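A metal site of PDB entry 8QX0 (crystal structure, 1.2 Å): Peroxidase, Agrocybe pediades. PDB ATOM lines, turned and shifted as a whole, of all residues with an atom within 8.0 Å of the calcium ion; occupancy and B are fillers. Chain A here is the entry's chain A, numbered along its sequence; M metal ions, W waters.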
ATOM      1  N   LEU A  43      36.830 -22.953  23.716  1.00  0.00           N
ATOM      2  CA  LEU A  43      36.321 -21.719  23.140  1.00  0.00           C
ATOM      3  C   LEU A  43      35.225 -22.012  22.104  1.00  0.00           C
ATOM      4  O   LEU A  43      34.288 -21.225  21.973  1.00  0.00           O
ATOM      5  CB  LEU A  43      37.492 -20.940  22.549  1.00  0.00           C
ATOM      6  CG  LEU A  43      37.201 -19.495  22.186  1.00  0.00           C
ATOM      7  CD1 LEU A  43      36.897 -18.688  23.419  1.00  0.00           C
ATOM      8  CD2 LEU A  43      38.419 -18.940  21.438  1.00  0.00           C
ATOM      9  N   VAL A  44      35.312 -23.148  21.394  1.00  0.00           N
ATOM     10  CA  VAL A  44      34.242 -23.549  20.491  1.00  0.00           C
ATOM     11  C   VAL A  44      32.904 -23.580  21.216  1.00  0.00           C
ATOM     12  O   VAL A  44      31.893 -23.036  20.722  1.00  0.00           O
ATOM     13  CB  VAL A  44      34.572 -24.923  19.903  1.00  0.00           C
ATOM     14  CG1 VAL A  44      33.379 -25.615  19.232  1.00  0.00           C
ATOM     15  CG2 VAL A  44      35.710 -24.860  18.919  1.00  0.00           C
ATOM     16  N   PHE A  45      32.886 -24.265  22.375  1.00  0.00           N
ATOM     17  CA  PHE A  45      31.665 -24.378  23.158  1.00  0.00           C
ATOM     18  C   PHE A  45      31.156 -23.030  23.633  1.00  0.00           C
ATOM     19  O   PHE A  45      29.988 -22.707  23.501  1.00  0.00           O
ATOM     20  CB  PHE A  45      31.969 -25.336  24.312  1.00  0.00           C
ATOM     21  CG  PHE A  45      30.817 -25.611  25.251  1.00  0.00           C
ATOM     22  CD1 PHE A  45      29.590 -26.022  24.756  1.00  0.00           C
ATOM     23  CD2 PHE A  45      30.962 -25.404  26.606  1.00  0.00           C
ATOM     24  CE1 PHE A  45      28.565 -26.286  25.647  1.00  0.00           C
ATOM     25  CE2 PHE A  45      29.891 -25.641  27.486  1.00  0.00           C
ATOM     26  CZ  PHE A  45      28.719 -26.085  26.962  1.00  0.00           C
ATOM     27  N   HIS A  46      32.007 -22.235  24.283  1.00  0.00           N
ATOM     28  CA  HIS A  46      31.562 -21.012  24.881  1.00  0.00           C
ATOM     29  C   HIS A  46      31.116 -19.971  23.843  1.00  0.00           C
ATOM     30  O   HIS A  46      30.255 -19.114  24.119  1.00  0.00           O
ATOM     31  CB  HIS A  46      32.652 -20.448  25.816  1.00  0.00           C
ATOM     32  CG  HIS A  46      32.823 -21.275  27.046  1.00  0.00           C
ATOM     33  ND1 HIS A  46      32.412 -20.784  28.281  1.00  0.00           N
ATOM     34  CD2 HIS A  46      33.222 -22.532  27.244  1.00  0.00           C
ATOM     35  CE1 HIS A  46      32.599 -21.742  29.205  1.00  0.00           C
ATOM     36  NE2 HIS A  46      33.089 -22.821  28.630  1.00  0.00           N
ATOM     37  N   ASP A  47      31.712 -20.035  22.662  1.00  0.00           N
ATOM     38  CA  ASP A  47      31.199 -19.231  21.573  1.00  0.00           C
ATOM     39  C   ASP A  47      29.862 -19.774  21.064  1.00  0.00           C
ATOM     40  O   ASP A  47      28.879 -19.031  21.010  1.00  0.00           O
ATOM     41  CB  ASP A  47      32.152 -19.138  20.389  1.00  0.00           C
ATOM     42  CG  ASP A  47      31.758 -18.011  19.443  1.00  0.00           C
ATOM     43  OD1 ASP A  47      31.004 -17.072  19.860  1.00  0.00           O
ATOM     44  OD2 ASP A  47      32.196 -18.070  18.273  1.00  0.00           O
ATOM     45  N   ALA A  48      29.839 -21.047  20.670  1.00  0.00           N
ATOM     46  CA  ALA A  48      28.740 -21.568  19.847  1.00  0.00           C
ATOM     47  C   ALA A  48      27.476 -21.838  20.654  1.00  0.00           C
ATOM     48  O   ALA A  48      26.408 -21.666  20.105  1.00  0.00           O
ATOM     49  CB  ALA A  48      29.194 -22.840  19.160  1.00  0.00           C
ATOM     50  N   ILE A  49      27.596 -22.336  21.887  1.00  0.00           N
ATOM     51  CA  ILE A  49      26.408 -22.798  22.617  1.00  0.00           C
ATOM     52  C   ILE A  49      25.558 -21.625  23.073  1.00  0.00           C
ATOM     53  O   ILE A  49      24.421 -21.826  23.466  1.00  0.00           O
ATOM     54  CB  ILE A  49      26.785 -23.723  23.799  1.00  0.00           C
ATOM     55  CG1 ILE A  49      25.633 -24.707  24.119  1.00  0.00           C
ATOM     56  CG2 ILE A  49      27.208 -22.952  25.000  1.00  0.00           C
ATOM     57  CD1 ILE A  49      25.499 -25.806  23.113  1.00  0.00           C
ATOM     58  N   ALA A  50      26.088 -20.396  23.041  1.00  0.00           N
ATOM     59  CA  ALA A  50      25.423 -19.237  23.609  1.00  0.00           C
ATOM     60  C   ALA A  50      24.435 -18.682  22.603  1.00  0.00           C
ATOM     61  O   ALA A  50      24.571 -17.583  22.060  1.00  0.00           O
ATOM     62  CB  ALA A  50      26.477 -18.214  24.036  1.00  0.00           C
ATOM     63  N   ILE A  51      23.383 -19.493  22.435  1.00  0.00           N
ATOM     64  CA  ILE A  51      22.255 -19.192  21.553  1.00  0.00           C
ATOM     65  C   ILE A  51      21.036 -19.930  22.121  1.00  0.00           C
ATOM     66  O   ILE A  51      21.186 -21.030  22.610  1.00  0.00           O
ATOM     67  CB  ILE A  51      22.517 -19.608  20.103  1.00  0.00           C
ATOM     68  CG1 ILE A  51      21.294 -19.392  19.197  1.00  0.00           C
ATOM     69  CG2 ILE A  51      23.030 -21.036  19.996  1.00  0.00           C
ATOM     70  CD1 ILE A  51      21.713 -19.528  17.726  1.00  0.00           C
ATOM     71  N   GLY A  57      21.077 -14.525  21.242  1.00  0.00           N
ATOM     72  CA  GLY A  57      22.447 -14.963  20.967  1.00  0.00           C
ATOM     73  C   GLY A  57      22.642 -15.411  19.535  1.00  0.00           C
ATOM     74  O   GLY A  57      21.796 -16.095  18.950  1.00  0.00           O
ATOM     75  N   GLY A  58      23.843 -15.186  18.991  1.00  0.00           N
ATOM     76  CA  GLY A  58      24.135 -15.508  17.614  1.00  0.00           C
ATOM     77  C   GLY A  58      24.771 -16.880  17.402  1.00  0.00           C
ATOM     78  O   GLY A  58      25.031 -17.276  16.281  1.00  0.00           O
ATOM     79  N   GLY A  59      25.170 -17.570  18.453  1.00  0.00           N
ATOM     80  CA  GLY A  59      25.748 -18.893  18.274  1.00  0.00           C
ATOM     81  C   GLY A  59      27.234 -18.851  17.895  1.00  0.00           C
ATOM     82  O   GLY A  59      27.992 -18.097  18.511  1.00  0.00           O
ATOM     83  N   ALA A  60      27.610 -19.594  16.879  1.00  0.00           N
ATOM     84  CA  ALA A  60      28.993 -19.724  16.408  1.00  0.00           C
ATOM     85  C   ALA A  60      29.301 -18.481  15.578  1.00  0.00           C
ATOM     86  O   ALA A  60      29.350 -18.552  14.339  1.00  0.00           O
ATOM     87  CB  ALA A  60      29.179 -21.013  15.645  1.00  0.00           C
ATOM     88  N   ASP A  61      29.480 -17.352  16.228  1.00  0.00           N
ATOM     89  CA  ASP A  61      29.528 -16.057  15.571  1.00  0.00           C
ATOM     90  C   ASP A  61      30.777 -15.256  15.961  1.00  0.00           C
ATOM     91  O   ASP A  61      30.924 -14.142  15.481  1.00  0.00           O
ATOM     92  CB  ASP A  61      28.279 -15.240  15.914  1.00  0.00           C
ATOM     93  CG  ASP A  61      28.090 -14.901  17.373  1.00  0.00           C
ATOM     94  OD1 ASP A  61      28.785 -15.431  18.233  1.00  0.00           O
ATOM     95  OD2 ASP A  61      27.143 -14.099  17.675  1.00  0.00           O
ATOM     96  N   GLY A  62      31.649 -15.774  16.826  1.00  0.00           N
ATOM     97  CA  GLY A  62      32.786 -15.006  17.285  1.00  0.00           C
ATOM     98  C   GLY A  62      32.495 -14.000  18.378  1.00  0.00           C
ATOM     99  O   GLY A  62      33.360 -13.217  18.769  1.00  0.00           O
ATOM    100  N   SER A  63      31.255 -13.987  18.911  1.00  0.00           N
ATOM    101  CA  SER A  63      30.854 -12.991  19.886  1.00  0.00           C
ATOM    102  C   SER A  63      31.708 -13.056  21.138  1.00  0.00           C
ATOM    103  O   SER A  63      31.961 -12.000  21.756  1.00  0.00           O
ATOM    104  CB  SER A  63      29.419 -13.149  20.231  1.00  0.00           C
ATOM    105  OG  SER A  63      29.152 -14.363  20.966  1.00  0.00           O
ATOM    106  N   ILE A  64      32.103 -14.224  21.577  1.00  0.00           N
ATOM    107  CA  ILE A  64      32.886 -14.393  22.795  1.00  0.00           C
ATOM    108  C   ILE A  64      34.196 -13.603  22.690  1.00  0.00           C
ATOM    109  O   ILE A  64      34.767 -13.223  23.711  1.00  0.00           O
ATOM    110  CB  ILE A  64      33.126 -15.878  23.149  1.00  0.00           C
ATOM    111  CG1 ILE A  64      33.768 -16.078  24.504  1.00  0.00           C
ATOM    112  CG2 ILE A  64      34.020 -16.604  22.177  1.00  0.00           C
ATOM    113  CD1 ILE A  64      32.843 -16.061  25.674  1.00  0.00           C
ATOM    114  N   ALA A  65      34.762 -13.489  21.473  1.00  0.00           N
ATOM    115  CA  ALA A  65      35.958 -12.688  21.288  1.00  0.00           C
ATOM    116  C   ALA A  65      35.653 -11.215  21.020  1.00  0.00           C
ATOM    117  O   ALA A  65      36.151 -10.344  21.745  1.00  0.00           O
ATOM    118  CB  ALA A  65      36.752 -13.285  20.156  1.00  0.00           C
ATOM    119  N   PHE A  67      32.970  -9.417  21.569  1.00  0.00           N
ATOM    120  CA  PHE A  67      32.221  -8.833  22.680  1.00  0.00           C
ATOM    121  C   PHE A  67      32.686  -9.414  24.001  1.00  0.00           C
ATOM    122  O   PHE A  67      31.884  -9.537  24.932  1.00  0.00           O
ATOM    123  CB  PHE A  67      30.746  -8.969  22.413  1.00  0.00           C
ATOM    124  CG  PHE A  67      30.286  -8.318  21.126  1.00  0.00           C
ATOM    125  CD1 PHE A  67      30.380  -6.957  20.951  1.00  0.00           C
ATOM    126  CD2 PHE A  67      29.800  -9.065  20.082  1.00  0.00           C
ATOM    127  CE1 PHE A  67      29.940  -6.367  19.775  1.00  0.00           C
ATOM    128  CE2 PHE A  67      29.379  -8.458  18.922  1.00  0.00           C
ATOM    129  CZ  PHE A  67      29.478  -7.131  18.739  1.00  0.00           C
ATOM    130  N   GLU A  71      30.886 -10.573  27.472  1.00  0.00           N
ATOM    131  CA  GLU A  71      30.706 -11.996  27.754  1.00  0.00           C
ATOM    132  C   GLU A  71      31.640 -12.482  28.879  1.00  0.00           C
ATOM    133  O   GLU A  71      31.296 -13.492  29.552  1.00  0.00           O
ATOM    134  CB  GLU A  71      30.816 -12.849  26.479  1.00  0.00           C
ATOM    135  CG  GLU A  71      29.713 -12.554  25.464  1.00  0.00           C
ATOM    136  CD  GLU A  71      29.557 -13.574  24.353  1.00  0.00           C
ATOM    137  OE1 GLU A  71      29.927 -14.779  24.568  1.00  0.00           O
ATOM    138  OE2 GLU A  71      28.992 -13.191  23.307  1.00  0.00           O
ATOM    139  N   GLY A 101      34.046 -15.791  14.080  1.00  0.00           N
ATOM    140  CA  GLY A 101      33.339 -17.048  14.272  1.00  0.00           C
ATOM    141  C   GLY A 101      34.031 -18.165  13.503  1.00  0.00           C
ATOM    142  O   GLY A 101      34.147 -19.274  13.986  1.00  0.00           O
ATOM    143  N   ILE A 104      37.333 -19.177  15.299  1.00  0.00           N
ATOM    144  CA  ILE A 104      37.181 -19.989  16.482  1.00  0.00           C
ATOM    145  C   ILE A 104      36.904 -21.439  16.102  1.00  0.00           C
ATOM    146  O   ILE A 104      37.438 -22.384  16.688  1.00  0.00           O
ATOM    147  CB  ILE A 104      36.121 -19.403  17.438  1.00  0.00           C
ATOM    148  CG1 ILE A 104      36.661 -18.140  18.088  1.00  0.00           C
ATOM    149  CG2 ILE A 104      35.680 -20.428  18.475  1.00  0.00           C
ATOM    150  CD1 ILE A 104      35.694 -17.384  18.967  1.00  0.00           C
ATOM    151  N   GLN A 105      36.041 -21.673  15.104  1.00  0.00           N
ATOM    152  CA  GLN A 105      35.767 -23.035  14.686  1.00  0.00           C
ATOM    153  C   GLN A 105      36.989 -23.702  14.045  1.00  0.00           C
ATOM    154  O   GLN A 105      37.243 -24.897  14.256  1.00  0.00           O
ATOM    155  CB  GLN A 105      34.538 -23.095  13.753  1.00  0.00           C
ATOM    156  CG  GLN A 105      33.271 -22.635  14.453  1.00  0.00           C
ATOM    157  CD  GLN A 105      32.987 -23.423  15.728  1.00  0.00           C
ATOM    158  OE1 GLN A 105      33.133 -24.640  15.776  1.00  0.00           O
ATOM    159  NE2 GLN A 105      32.545 -22.726  16.775  1.00  0.00           N
ATOM    160  N   PRO A 130      29.780 -11.042  14.260  1.00  0.00           N
ATOM    161  CA  PRO A 130      28.705 -11.046  15.258  1.00  0.00           C
ATOM    162  C   PRO A 130      28.049  -9.672  15.383  1.00  0.00           C
ATOM    163  O   PRO A 130      28.697  -8.618  15.225  1.00  0.00           O
ATOM    164  CB  PRO A 130      29.478 -11.468  16.522  1.00  0.00           C
ATOM    165  CG  PRO A 130      30.850 -10.866  16.314  1.00  0.00           C
ATOM    166  CD  PRO A 130      31.123 -11.040  14.865  1.00  0.00           C
ATOM    167  N   ALA A 132      26.031  -8.783  18.333  1.00  0.00           N
ATOM    168  CA  ALA A 132      25.932  -8.410  19.729  1.00  0.00           C
ATOM    169  C   ALA A 132      26.456  -9.536  20.597  1.00  0.00           C
ATOM    170  O   ALA A 132      26.471 -10.710  20.190  1.00  0.00           O
ATOM    171  CB  ALA A 132      24.515  -8.060  20.091  1.00  0.00           C
ATOM    172  N   ALA A 133      26.792  -9.187  21.829  1.00  0.00           N
ATOM    173  CA  ALA A 133      27.098 -10.195  22.848  1.00  0.00           C
ATOM    174  C   ALA A 133      25.926 -11.165  22.958  1.00  0.00           C
ATOM    175  O   ALA A 133      24.752 -10.755  22.928  1.00  0.00           O
ATOM    176  CB  ALA A 133      27.342  -9.493  24.178  1.00  0.00           C
ATOM    177  N   ALA A 134      26.261 -12.398  23.314  1.00  0.00           N
ATOM    178  CA  ALA A 134      25.258 -13.349  23.775  1.00  0.00           C
ATOM    179  C   ALA A 134      24.610 -12.803  25.044  1.00  0.00           C
ATOM    180  O   ALA A 134      25.269 -12.196  25.903  1.00  0.00           O
ATOM    181  CB  ALA A 134      25.890 -14.664  24.073  1.00  0.00           C
ATOM    182  N   VAL A 139      25.393 -20.366  28.642  1.00  0.00           N
ATOM    183  CA  VAL A 139      26.407 -21.398  28.695  1.00  0.00           C
ATOM    184  C   VAL A 139      26.127 -22.270  29.903  1.00  0.00           C
ATOM    185  O   VAL A 139      26.100 -21.749  31.014  1.00  0.00           O
ATOM    186  CB  VAL A 139      27.810 -20.802  28.766  1.00  0.00           C
ATOM    187  CG1 VAL A 139      28.848 -21.912  28.850  1.00  0.00           C
ATOM    188  CG2 VAL A 139      28.089 -19.925  27.535  1.00  0.00           C
ATOM    189  N   LEU A 270      25.780 -23.591  14.763  1.00  0.00           N
ATOM    190  CA  LEU A 270      24.726 -22.976  15.536  1.00  0.00           C
ATOM    191  C   LEU A 270      24.652 -21.499  15.166  1.00  0.00           C
ATOM    192  O   LEU A 270      25.627 -20.773  15.107  1.00  0.00           O
ATOM    193  CB  LEU A 270      24.969 -23.151  17.034  1.00  0.00           C
ATOM    194  CG  LEU A 270      24.822 -24.587  17.526  1.00  0.00           C
ATOM    195  CD1 LEU A 270      25.313 -24.735  18.931  1.00  0.00           C
ATOM    196  CD2 LEU A 270      23.347 -24.970  17.450  1.00  0.00           C
HETATM  197 CA    CA M   1      28.796 -16.685  20.310  1.00  0.00          CA
HETATM  198  O   HOH W   1      29.349 -16.644  22.691  1.00  0.00           O
HETATM  199  O   HOH W   2      26.564 -16.140  20.884  1.00  0.00           O
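The side-chain carboxylate of Asp 47 is in hydrogen-bond range of the backbone NH of Gly 62 (2.8 Å).
The side-chain carboxylate of Glu 71 lies close to the side-chain hydroxyl of Ser 63 (2.6 Å).
Of the 29 residues printed, 4 come within 4 Å of the calcium ion.
The calcium ion is bound by OD1 of Asp 47 (2.3 Å), water W2 (2.4 Å), O of Gly 59 (2.4 Å), OD1 of Asp 61 (2.4 Å), OG of Ser 63 (2.4 Å), water W1 (2.4 Å) and O of Asp 47 (2.4 Å).
The calcium ion has seven donor atoms within binding distance.
Water W1 bridges the side-chain carboxylate (OE1) of Glu 71 (2.7 Å) and the backbone carbonyl oxygen (O) of His 46 (3.0 Å).
Water W2 lies within hydrogen-bond range of O of Ala 50, N of Gly 59 and N of Gly 58.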
